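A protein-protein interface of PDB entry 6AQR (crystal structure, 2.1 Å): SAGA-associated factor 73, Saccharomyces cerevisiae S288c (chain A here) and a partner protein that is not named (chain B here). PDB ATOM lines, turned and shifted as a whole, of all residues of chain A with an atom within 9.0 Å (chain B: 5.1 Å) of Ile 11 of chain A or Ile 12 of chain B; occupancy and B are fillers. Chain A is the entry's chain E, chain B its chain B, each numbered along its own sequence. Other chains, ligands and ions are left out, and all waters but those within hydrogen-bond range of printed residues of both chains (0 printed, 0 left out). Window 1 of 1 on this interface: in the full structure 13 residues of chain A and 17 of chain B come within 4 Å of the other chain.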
ATOM      1  N   ILE A   8      16.182 -11.887  27.386  1.00  0.00           N
ATOM      2  CA  ILE A   8      15.225 -12.374  26.370  1.00  0.00           C
ATOM      3  C   ILE A   8      13.907 -11.611  26.426  1.00  0.00           C
ATOM      4  O   ILE A   8      13.158 -11.722  27.405  1.00  0.00           O
ATOM      5  CB  ILE A   8      14.958 -13.905  26.503  1.00  0.00           C
ATOM      6  CG1 ILE A   8      16.260 -14.680  26.241  1.00  0.00           C
ATOM      7  CG2 ILE A   8      13.827 -14.364  25.576  1.00  0.00           C
ATOM      8  CD1 ILE A   8      16.206 -16.165  26.510  1.00  0.00           C
ATOM      9  N   LYS A   9      13.632 -10.861  25.354  1.00  0.00           N
ATOM     10  CA  LYS A   9      12.404 -10.064  25.229  1.00  0.00           C
ATOM     11  C   LYS A   9      11.195 -10.962  24.917  1.00  0.00           C
ATOM     12  O   LYS A   9      10.134 -10.846  25.557  1.00  0.00           O
ATOM     13  CB  LYS A   9      12.576  -8.936  24.189  1.00  0.00           C
ATOM     14  CG  LYS A   9      13.860  -8.104  24.339  1.00  0.00           C
ATOM     15  CD  LYS A   9      13.811  -6.759  23.613  1.00  0.00           C
ATOM     16  CE  LYS A   9      13.316  -5.635  24.549  1.00  0.00           C
ATOM     17  NZ  LYS A   9      13.482  -4.244  24.010  1.00  0.00           N
ATOM     18  N   GLY A  10      11.386 -11.866  23.949  1.00  0.00           N
ATOM     19  CA  GLY A  10      10.380 -12.854  23.511  1.00  0.00           C
ATOM     20  C   GLY A  10      10.918 -13.661  22.337  1.00  0.00           C
ATOM     21  O   GLY A  10      12.066 -13.471  21.906  1.00  0.00           O
ATOM     22  N   ILE A  11      10.089 -14.554  21.807  1.00  0.00           N
ATOM     23  CA  ILE A  11      10.452 -15.355  20.617  1.00  0.00           C
ATOM     24  C   ILE A  11      10.219 -14.481  19.373  1.00  0.00           C
ATOM     25  O   ILE A  11       9.199 -13.790  19.328  1.00  0.00           O
ATOM     26  CB  ILE A  11       9.625 -16.674  20.595  1.00  0.00           C
ATOM     27  CG1 ILE A  11      10.217 -17.678  21.600  1.00  0.00           C
ATOM     28  CG2 ILE A  11       9.595 -17.314  19.222  1.00  0.00           C
ATOM     29  CD1 ILE A  11       9.154 -18.423  22.426  1.00  0.00           C
ATOM     30  N   LYS A  12      11.140 -14.492  18.393  1.00  0.00           N
ATOM     31  CA  LYS A  12      10.941 -13.786  17.101  1.00  0.00           C
ATOM     32  C   LYS A  12       9.585 -14.114  16.496  1.00  0.00           C
ATOM     33  O   LYS A  12       9.232 -15.294  16.448  1.00  0.00           O
ATOM     34  CB  LYS A  12      12.046 -14.101  16.097  1.00  0.00           C
ATOM     35  CG  LYS A  12      13.384 -13.567  16.543  1.00  0.00           C
ATOM     36  CD  LYS A  12      14.513 -13.809  15.556  1.00  0.00           C
ATOM     37  CE  LYS A  12      15.743 -13.123  16.116  1.00  0.00           C
ATOM     38  NZ  LYS A  12      17.032 -13.580  15.547  1.00  0.00           N
ATOM     39  N   PRO A  13       8.800 -13.079  16.067  1.00  0.00           N
ATOM     40  CA  PRO A  13       7.411 -13.401  15.662  1.00  0.00           C
ATOM     41  C   PRO A  13       7.407 -14.078  14.271  1.00  0.00           C
ATOM     42  O   PRO A  13       6.474 -14.837  13.935  1.00  0.00           O
ATOM     43  CB  PRO A  13       6.707 -12.036  15.668  1.00  0.00           C
ATOM     44  CG  PRO A  13       7.804 -11.023  15.464  1.00  0.00           C
ATOM     45  CD  PRO A  13       9.146 -11.662  15.774  1.00  0.00           C
ATOM     46  N   LYS A  14       8.468 -13.797  13.501  1.00  0.00           N
ATOM     47  CA  LYS A  14       8.874 -14.555  12.310  1.00  0.00           C
ATOM     48  C   LYS A  14       8.857 -16.058  12.611  1.00  0.00           C
ATOM     49  O   LYS A  14       8.328 -16.830  11.829  1.00  0.00           O
ATOM     50  CB  LYS A  14      10.303 -14.160  11.854  1.00  0.00           C
ATOM     51  CG  LYS A  14      10.888 -12.856  12.437  1.00  0.00           C
ATOM     52  CD  LYS A  14      12.343 -12.657  12.009  1.00  0.00           C
ATOM     53  CE  LYS A  14      12.823 -11.218  12.190  1.00  0.00           C
ATOM     54  NZ  LYS A  14      13.347 -10.946  13.555  1.00  0.00           N
ATOM     55  N   VAL A  15       9.407 -16.449  13.770  1.00  0.00           N
ATOM     56  CA  VAL A  15       9.580 -17.854  14.171  1.00  0.00           C
ATOM     57  C   VAL A  15       8.288 -18.508  14.672  1.00  0.00           C
ATOM     58  O   VAL A  15       8.014 -19.663  14.295  1.00  0.00           O
ATOM     59  CB  VAL A  15      10.819 -18.018  15.113  1.00  0.00           C
ATOM     60  CG1 VAL A  15      10.792 -19.310  15.938  1.00  0.00           C
ATOM     61  CG2 VAL A  15      12.105 -17.942  14.293  1.00  0.00           C
ATOM     62  N   ILE A  16       7.493 -17.774  15.474  1.00  0.00           N
ATOM     63  CA  ILE A  16       6.180 -18.251  16.018  1.00  0.00           C
ATOM     64  C   ILE A  16       5.206 -18.597  14.897  1.00  0.00           C
ATOM     65  O   ILE A  16       4.338 -19.463  15.066  1.00  0.00           O
ATOM     66  CB  ILE A  16       5.480 -17.249  17.005  1.00  0.00           C
ATOM     67  CG1 ILE A  16       6.362 -16.943  18.227  1.00  0.00           C
ATOM     68  CG2 ILE A  16       4.142 -17.795  17.518  1.00  0.00           C
ATOM     69  CD1 ILE A  16       5.892 -15.803  19.130  1.00  0.00           C
ATOM     70  N   GLU A  17       5.361 -17.920  13.760  1.00  0.00           N
ATOM     71  CA  GLU A  17       4.539 -18.169  12.565  1.00  0.00           C
ATOM     72  C   GLU A  17       4.910 -19.500  11.857  1.00  0.00           C
ATOM     73  O   GLU A  17       4.041 -20.344  11.602  1.00  0.00           O
ATOM     74  CB  GLU A  17       4.598 -16.937  11.629  1.00  0.00           C
ATOM     75  CG  GLU A  17       3.797 -17.013  10.325  1.00  0.00           C
ATOM     76  CD  GLU A  17       2.288 -16.840  10.498  1.00  0.00           C
ATOM     77  OE1 GLU A  17       1.832 -16.455  11.604  1.00  0.00           O
ATOM     78  OE2 GLU A  17       1.554 -17.092   9.512  1.00  0.00           O
ATOM     79  N   GLU A  18       6.203 -19.690  11.599  1.00  0.00           N
ATOM     80  CA  GLU A  18       6.746 -20.847  10.879  1.00  0.00           C
ATOM     81  C   GLU A  18       6.520 -22.224  11.527  1.00  0.00           C
ATOM     82  O   GLU A  18       6.703 -23.252  10.861  1.00  0.00           O
ATOM     83  CB  GLU A  18       8.250 -20.618  10.615  1.00  0.00           C
ATOM     84  CG  GLU A  18       8.602 -19.897   9.306  1.00  0.00           C
ATOM     85  CD  GLU A  18       8.108 -18.436   9.174  1.00  0.00           C
ATOM     86  OE1 GLU A  18       7.056 -18.044   9.753  1.00  0.00           O
ATOM     87  OE2 GLU A  18       8.772 -17.650   8.447  1.00  0.00           O
ATOM     88  N   TYR A  19       6.086 -22.238  12.793  1.00  0.00           N
ATOM     89  CA  TYR A  19       6.154 -23.417  13.639  1.00  0.00           C
ATOM     90  C   TYR A  19       4.900 -23.632  14.484  1.00  0.00           C
ATOM     91  O   TYR A  19       4.786 -24.630  15.205  1.00  0.00           O
ATOM     92  CB  TYR A  19       7.411 -23.321  14.541  1.00  0.00           C
ATOM     93  CG  TYR A  19       8.734 -23.676  13.843  1.00  0.00           C
ATOM     94  CD1 TYR A  19       9.108 -25.020  13.664  1.00  0.00           C
ATOM     95  CD2 TYR A  19       9.603 -22.676  13.356  1.00  0.00           C
ATOM     96  CE1 TYR A  19      10.291 -25.361  13.014  1.00  0.00           C
ATOM     97  CE2 TYR A  19      10.800 -23.015  12.716  1.00  0.00           C
ATOM     98  CZ  TYR A  19      11.133 -24.367  12.552  1.00  0.00           C
ATOM     99  OH  TYR A  19      12.285 -24.773  11.936  1.00  0.00           O
ATOM    100  N   LEU A  21       3.887 -22.067  17.187  1.00  0.00           N
ATOM    101  CA  LEU A  21       4.277 -22.133  18.608  1.00  0.00           C
ATOM    102  C   LEU A  21       3.223 -21.463  19.514  1.00  0.00           C
ATOM    103  O   LEU A  21       2.057 -21.871  19.566  1.00  0.00           O
ATOM    104  CB  LEU A  21       5.679 -21.497  18.837  1.00  0.00           C
ATOM    105  CG  LEU A  21       6.987 -21.926  18.135  1.00  0.00           C
ATOM    106  CD1 LEU A  21       8.206 -21.080  18.493  1.00  0.00           C
ATOM    107  CD2 LEU A  21       7.304 -23.376  18.404  1.00  0.00           C
ATOM    108  N   LEU B   8       7.268 -19.685  28.095  1.00  0.00           N
ATOM    109  CA  LEU B   8       8.351 -19.368  27.203  1.00  0.00           C
ATOM    110  C   LEU B   8       9.273 -20.582  26.980  1.00  0.00           C
ATOM    111  O   LEU B   8       9.622 -20.889  25.831  1.00  0.00           O
ATOM    112  CB  LEU B   8       9.104 -18.141  27.708  1.00  0.00           C
ATOM    113  CG  LEU B   8      10.274 -17.695  26.823  1.00  0.00           C
ATOM    114  CD1 LEU B   8       9.787 -16.885  25.633  1.00  0.00           C
ATOM    115  CD2 LEU B   8      11.304 -16.916  27.636  1.00  0.00           C
ATOM    116  N   LYS B   9       9.635 -21.277  28.066  1.00  0.00           N
ATOM    117  CA  LYS B   9      10.656 -22.327  28.005  1.00  0.00           C
ATOM    118  C   LYS B   9      10.168 -23.506  27.159  1.00  0.00           C
ATOM    119  O   LYS B   9      10.925 -24.024  26.318  1.00  0.00           O
ATOM    120  CB  LYS B   9      11.107 -22.797  29.401  1.00  0.00           C
ATOM    121  CG  LYS B   9      12.240 -23.837  29.330  1.00  0.00           C
ATOM    122  CD  LYS B   9      12.770 -24.354  30.679  1.00  0.00           C
ATOM    123  CE  LYS B   9      14.186 -23.853  30.975  1.00  0.00           C
ATOM    124  NZ  LYS B   9      15.118 -23.919  29.802  1.00  0.00           N
ATOM    125  N   SER B  10       8.911 -23.893  27.378  1.00  0.00           N
ATOM    126  CA  SER B  10       8.278 -24.952  26.604  1.00  0.00           C
ATOM    127  C   SER B  10       8.155 -24.630  25.098  1.00  0.00           C
ATOM    128  O   SER B  10       8.464 -25.478  24.269  1.00  0.00           O
ATOM    129  CB  SER B  10       6.954 -25.391  27.229  1.00  0.00           C
ATOM    130  OG  SER B  10       6.022 -24.347  27.209  1.00  0.00           O
ATOM    131  N   GLN B  11       7.776 -23.397  24.739  1.00  0.00           N
ATOM    132  CA  GLN B  11       7.713 -22.991  23.328  1.00  0.00           C
ATOM    133  C   GLN B  11       9.043 -23.153  22.658  1.00  0.00           C
ATOM    134  O   GLN B  11       9.105 -23.683  21.543  1.00  0.00           O
ATOM    135  CB  GLN B  11       7.234 -21.560  23.137  1.00  0.00           C
ATOM    136  CG  GLN B  11       5.904 -21.274  23.811  1.00  0.00           C
ATOM    137  CD  GLN B  11       5.050 -20.214  23.126  1.00  0.00           C
ATOM    138  OE1 GLN B  11       3.823 -20.252  23.240  1.00  0.00           O
ATOM    139  NE2 GLN B  11       5.680 -19.275  22.409  1.00  0.00           N
ATOM    140  N   ILE B  12      10.103 -22.703  23.335  1.00  0.00           N
ATOM    141  CA  ILE B  12      11.447 -22.825  22.822  1.00  0.00           C
ATOM    142  C   ILE B  12      11.884 -24.291  22.615  1.00  0.00           C
ATOM    143  O   ILE B  12      12.498 -24.623  21.570  1.00  0.00           O
ATOM    144  CB  ILE B  12      12.448 -22.115  23.733  1.00  0.00           C
ATOM    145  CG1 ILE B  12      12.160 -20.613  23.781  1.00  0.00           C
ATOM    146  CG2 ILE B  12      13.869 -22.331  23.248  1.00  0.00           C
ATOM    147  CD1 ILE B  12      12.791 -19.936  24.986  1.00  0.00           C
ATOM    148  N   GLN B  13      11.602 -25.147  23.615  1.00  0.00           N
ATOM    149  CA  GLN B  13      11.895 -26.591  23.503  1.00  0.00           C
ATOM    150  C   GLN B  13      11.186 -27.187  22.326  1.00  0.00           C
ATOM    151  O   GLN B  13      11.802 -27.942  21.555  1.00  0.00           O
ATOM    152  CB  GLN B  13      11.516 -27.370  24.750  1.00  0.00           C
ATOM    153  CG  GLN B  13      12.510 -27.232  25.874  1.00  0.00           C
ATOM    154  CD  GLN B  13      11.897 -27.609  27.214  1.00  0.00           C
ATOM    155  OE1 GLN B  13      10.753 -28.047  27.302  1.00  0.00           O
ATOM    156  NE2 GLN B  13      12.665 -27.417  28.277  1.00  0.00           N
ATOM    157  N   GLN B  14       9.909 -26.832  22.178  1.00  0.00           N
ATOM    158  CA  GLN B  14       9.106 -27.265  21.043  1.00  0.00           C
ATOM    159  C   GLN B  14       9.739 -26.830  19.717  1.00  0.00           C
ATOM    160  O   GLN B  14       9.791 -27.611  18.779  1.00  0.00           O
ATOM    161  CB  GLN B  14       7.682 -26.741  21.135  1.00  0.00           C
ATOM    162  CG  GLN B  14       6.888 -26.990  19.857  1.00  0.00           C
ATOM    163  CD  GLN B  14       5.884 -28.105  20.041  1.00  0.00           C
ATOM    164  OE1 GLN B  14       5.564 -28.470  21.185  1.00  0.00           O
ATOM    165  NE2 GLN B  14       5.381 -28.663  18.929  1.00  0.00           N
ATOM    166  N   TYR B  15      10.247 -25.597  19.665  1.00  0.00           N
ATOM    167  CA  TYR B  15      10.942 -25.126  18.484  1.00  0.00           C
ATOM    168  C   TYR B  15      12.195 -26.008  18.200  1.00  0.00           C
ATOM    169  O   TYR B  15      12.523 -26.330  17.026  1.00  0.00           O
ATOM    170  CB  TYR B  15      11.359 -23.635  18.626  1.00  0.00           C
ATOM    171  CG  TYR B  15      12.461 -23.351  17.662  1.00  0.00           C
ATOM    172  CD1 TYR B  15      12.183 -23.162  16.298  1.00  0.00           C
ATOM    173  CD2 TYR B  15      13.796 -23.402  18.071  1.00  0.00           C
ATOM    174  CE1 TYR B  15      13.206 -22.968  15.385  1.00  0.00           C
ATOM    175  CE2 TYR B  15      14.824 -23.206  17.157  1.00  0.00           C
ATOM    176  CZ  TYR B  15      14.517 -23.006  15.826  1.00  0.00           C
ATOM    177  OH  TYR B  15      15.532 -22.831  14.934  1.00  0.00           O
ATOM    178  N   LEU B  16      12.941 -26.327  19.261  1.00  0.00           N
ATOM    179  CA  LEU B  16      14.224 -26.990  19.064  1.00  0.00           C
ATOM    180  C   LEU B  16      13.953 -28.417  18.548  1.00  0.00           C
ATOM    181  O   LEU B  16      14.686 -28.883  17.691  1.00  0.00           O
ATOM    182  CB  LEU B  16      15.042 -27.014  20.355  1.00  0.00           C
ATOM    183  CG  LEU B  16      15.692 -25.678  20.750  1.00  0.00           C
ATOM    184  CD1 LEU B  16      16.407 -25.843  22.085  1.00  0.00           C
ATOM    185  CD2 LEU B  16      16.666 -25.231  19.683  1.00  0.00           C
ATOM    186  N   LEU B  89      19.631 -20.785  20.252  1.00  0.00           N
ATOM    187  CA  LEU B  89      18.649 -19.874  20.838  1.00  0.00           C
ATOM    188  C   LEU B  89      18.690 -18.494  20.261  1.00  0.00           C
ATOM    189  O   LEU B  89      17.663 -17.817  20.254  1.00  0.00           O
ATOM    190  CB  LEU B  89      18.770 -19.784  22.354  1.00  0.00           C
ATOM    191  CG  LEU B  89      18.157 -20.934  23.130  1.00  0.00           C
ATOM    192  CD1 LEU B  89      17.888 -20.473  24.545  1.00  0.00           C
ATOM    193  CD2 LEU B  89      16.880 -21.453  22.472  1.00  0.00           C
ATOM    194  N   ILE B  92      16.248 -17.555  17.405  1.00  0.00           N
ATOM    195  CA  ILE B  92      14.785 -17.499  17.599  1.00  0.00           C
ATOM    196  C   ILE B  92      14.256 -16.632  18.750  1.00  0.00           C
ATOM    197  O   ILE B  92      13.043 -16.452  18.919  1.00  0.00           O
ATOM    198  CB  ILE B  92      14.157 -18.920  17.683  1.00  0.00           C
ATOM    199  CG1 ILE B  92      14.447 -19.585  19.039  1.00  0.00           C
ATOM    200  CG2 ILE B  92      14.589 -19.795  16.504  1.00  0.00           C
ATOM    201  CD1 ILE B  92      13.181 -20.150  19.648  1.00  0.00           C
ATOM    202  N   VAL B  93      15.158 -16.117  19.571  1.00  0.00           N
ATOM    203  CA  VAL B  93      14.720 -15.150  20.581  1.00  0.00           C
ATOM    204  C   VAL B  93      15.162 -13.728  20.240  1.00  0.00           C
ATOM    205  O   VAL B  93      16.206 -13.520  19.619  1.00  0.00           O
ATOM    206  CB  VAL B  93      15.129 -15.552  22.006  1.00  0.00           C
ATOM    207  CG1 VAL B  93      14.432 -16.858  22.375  1.00  0.00           C
ATOM    208  CG2 VAL B  93      16.653 -15.641  22.136  1.00  0.00           C
ATOM    209  N   ASP B  94      14.345 -12.760  20.643  1.00  0.00           N
ATOM    210  CA  ASP B  94      14.727 -11.344  20.559  1.00  0.00           C
ATOM    211  C   ASP B  94      15.551 -10.916  21.771  1.00  0.00           C
ATOM    212  O   ASP B  94      15.149 -11.172  22.922  1.00  0.00           O
ATOM    213  CB  ASP B  94      13.479 -10.454  20.455  1.00  0.00           C
ATOM    214  CG  ASP B  94      12.803 -10.528  19.093  1.00  0.00           C
ATOM    215  OD1 ASP B  94      13.503 -10.756  18.061  1.00  0.00           O
ATOM    216  OD2 ASP B  94      11.563 -10.341  19.068  1.00  0.00           O
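The backbone NH of Lys 9 of chain A is in hydrogen-bond range of the backbone carbonyl oxygen of Asp 94 of chain B, at 2.9 Å.
The backbone carbonyl oxygen (O) of Ile 92 of chain B sits at hydrogen-bond distance from the backbone NH (N) of Lys 12 of chain A, at 2.8 Å.
O of Gly 10 of chain A lies within hydrogen-bond range of N of Asp 94 of chain B, 2.7 Å away.
Ile 8 of chain A touches Val 93 of chain B.
CA of Ile 8 of chain A touches O of Asp 94 of chain B, at 3.7 Å.
Ile 11 of chain A touches Leu 8 of chain B (CD1 to CD1, 3.6 Å).
Gln 11 of chain B touches Ile 11 of chain A.
CE of Lys 12 of chain A touches O of Val 93 of chain B, at 3.6 Å.
Lys 12 of chain A touches Asp 94 of chain B.
Ile 92 of chain B touches Val 15 of chain A (CG2 to CG2, 3.8 Å).
Tyr 19 of chain A touches Tyr 15 of chain B.
Gln 11 of chain B touches Leu 21 of chain A.
CD2 of Leu 21 of chain A touches N of Tyr 15 of chain B, 3.9 Å away.
Of the printed residues of chain B, Gly 10 of chain A touches Val 93 and Asp 94.
Of chain B, only Leu 8 (3.6 Å), Gln 11 (3.6 Å), Ile 12 (3.96 Å) and Ile 92 (3.3 Å) come within 4 Å of Ile 11 of chain A.
Glu 17 of chain A touches none of the printed residues of chain B.
Of the printed residues of chain B, Leu 21 of chain A touches Gln 11 (3.6 Å), Gln 14 (3.9 Å) and Tyr 15 (3.9 Å).
Of chain A, only Ile 11 comes within 4 Å of Ile 12 of chain B.
Of the printed residues of chain A, Tyr 15 of chain B touches Tyr 19 (3.6 Å) and Leu 21 (3.9 Å).
Leu 89 of chain B touches none of the printed residues of chain A.
The nearest residue of chain B that does not touch Ile 11 of chain A is Asp 94 of chain B (4.2 Å).
The nearest residue of chain A that does not touch Ile 12 of chain B is Ile 8 of chain A (5.3 Å).
O of Ile 16 of chain A sits at hydrogen-bond distance from N of Leu 21 of chain A (3.4 Å).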
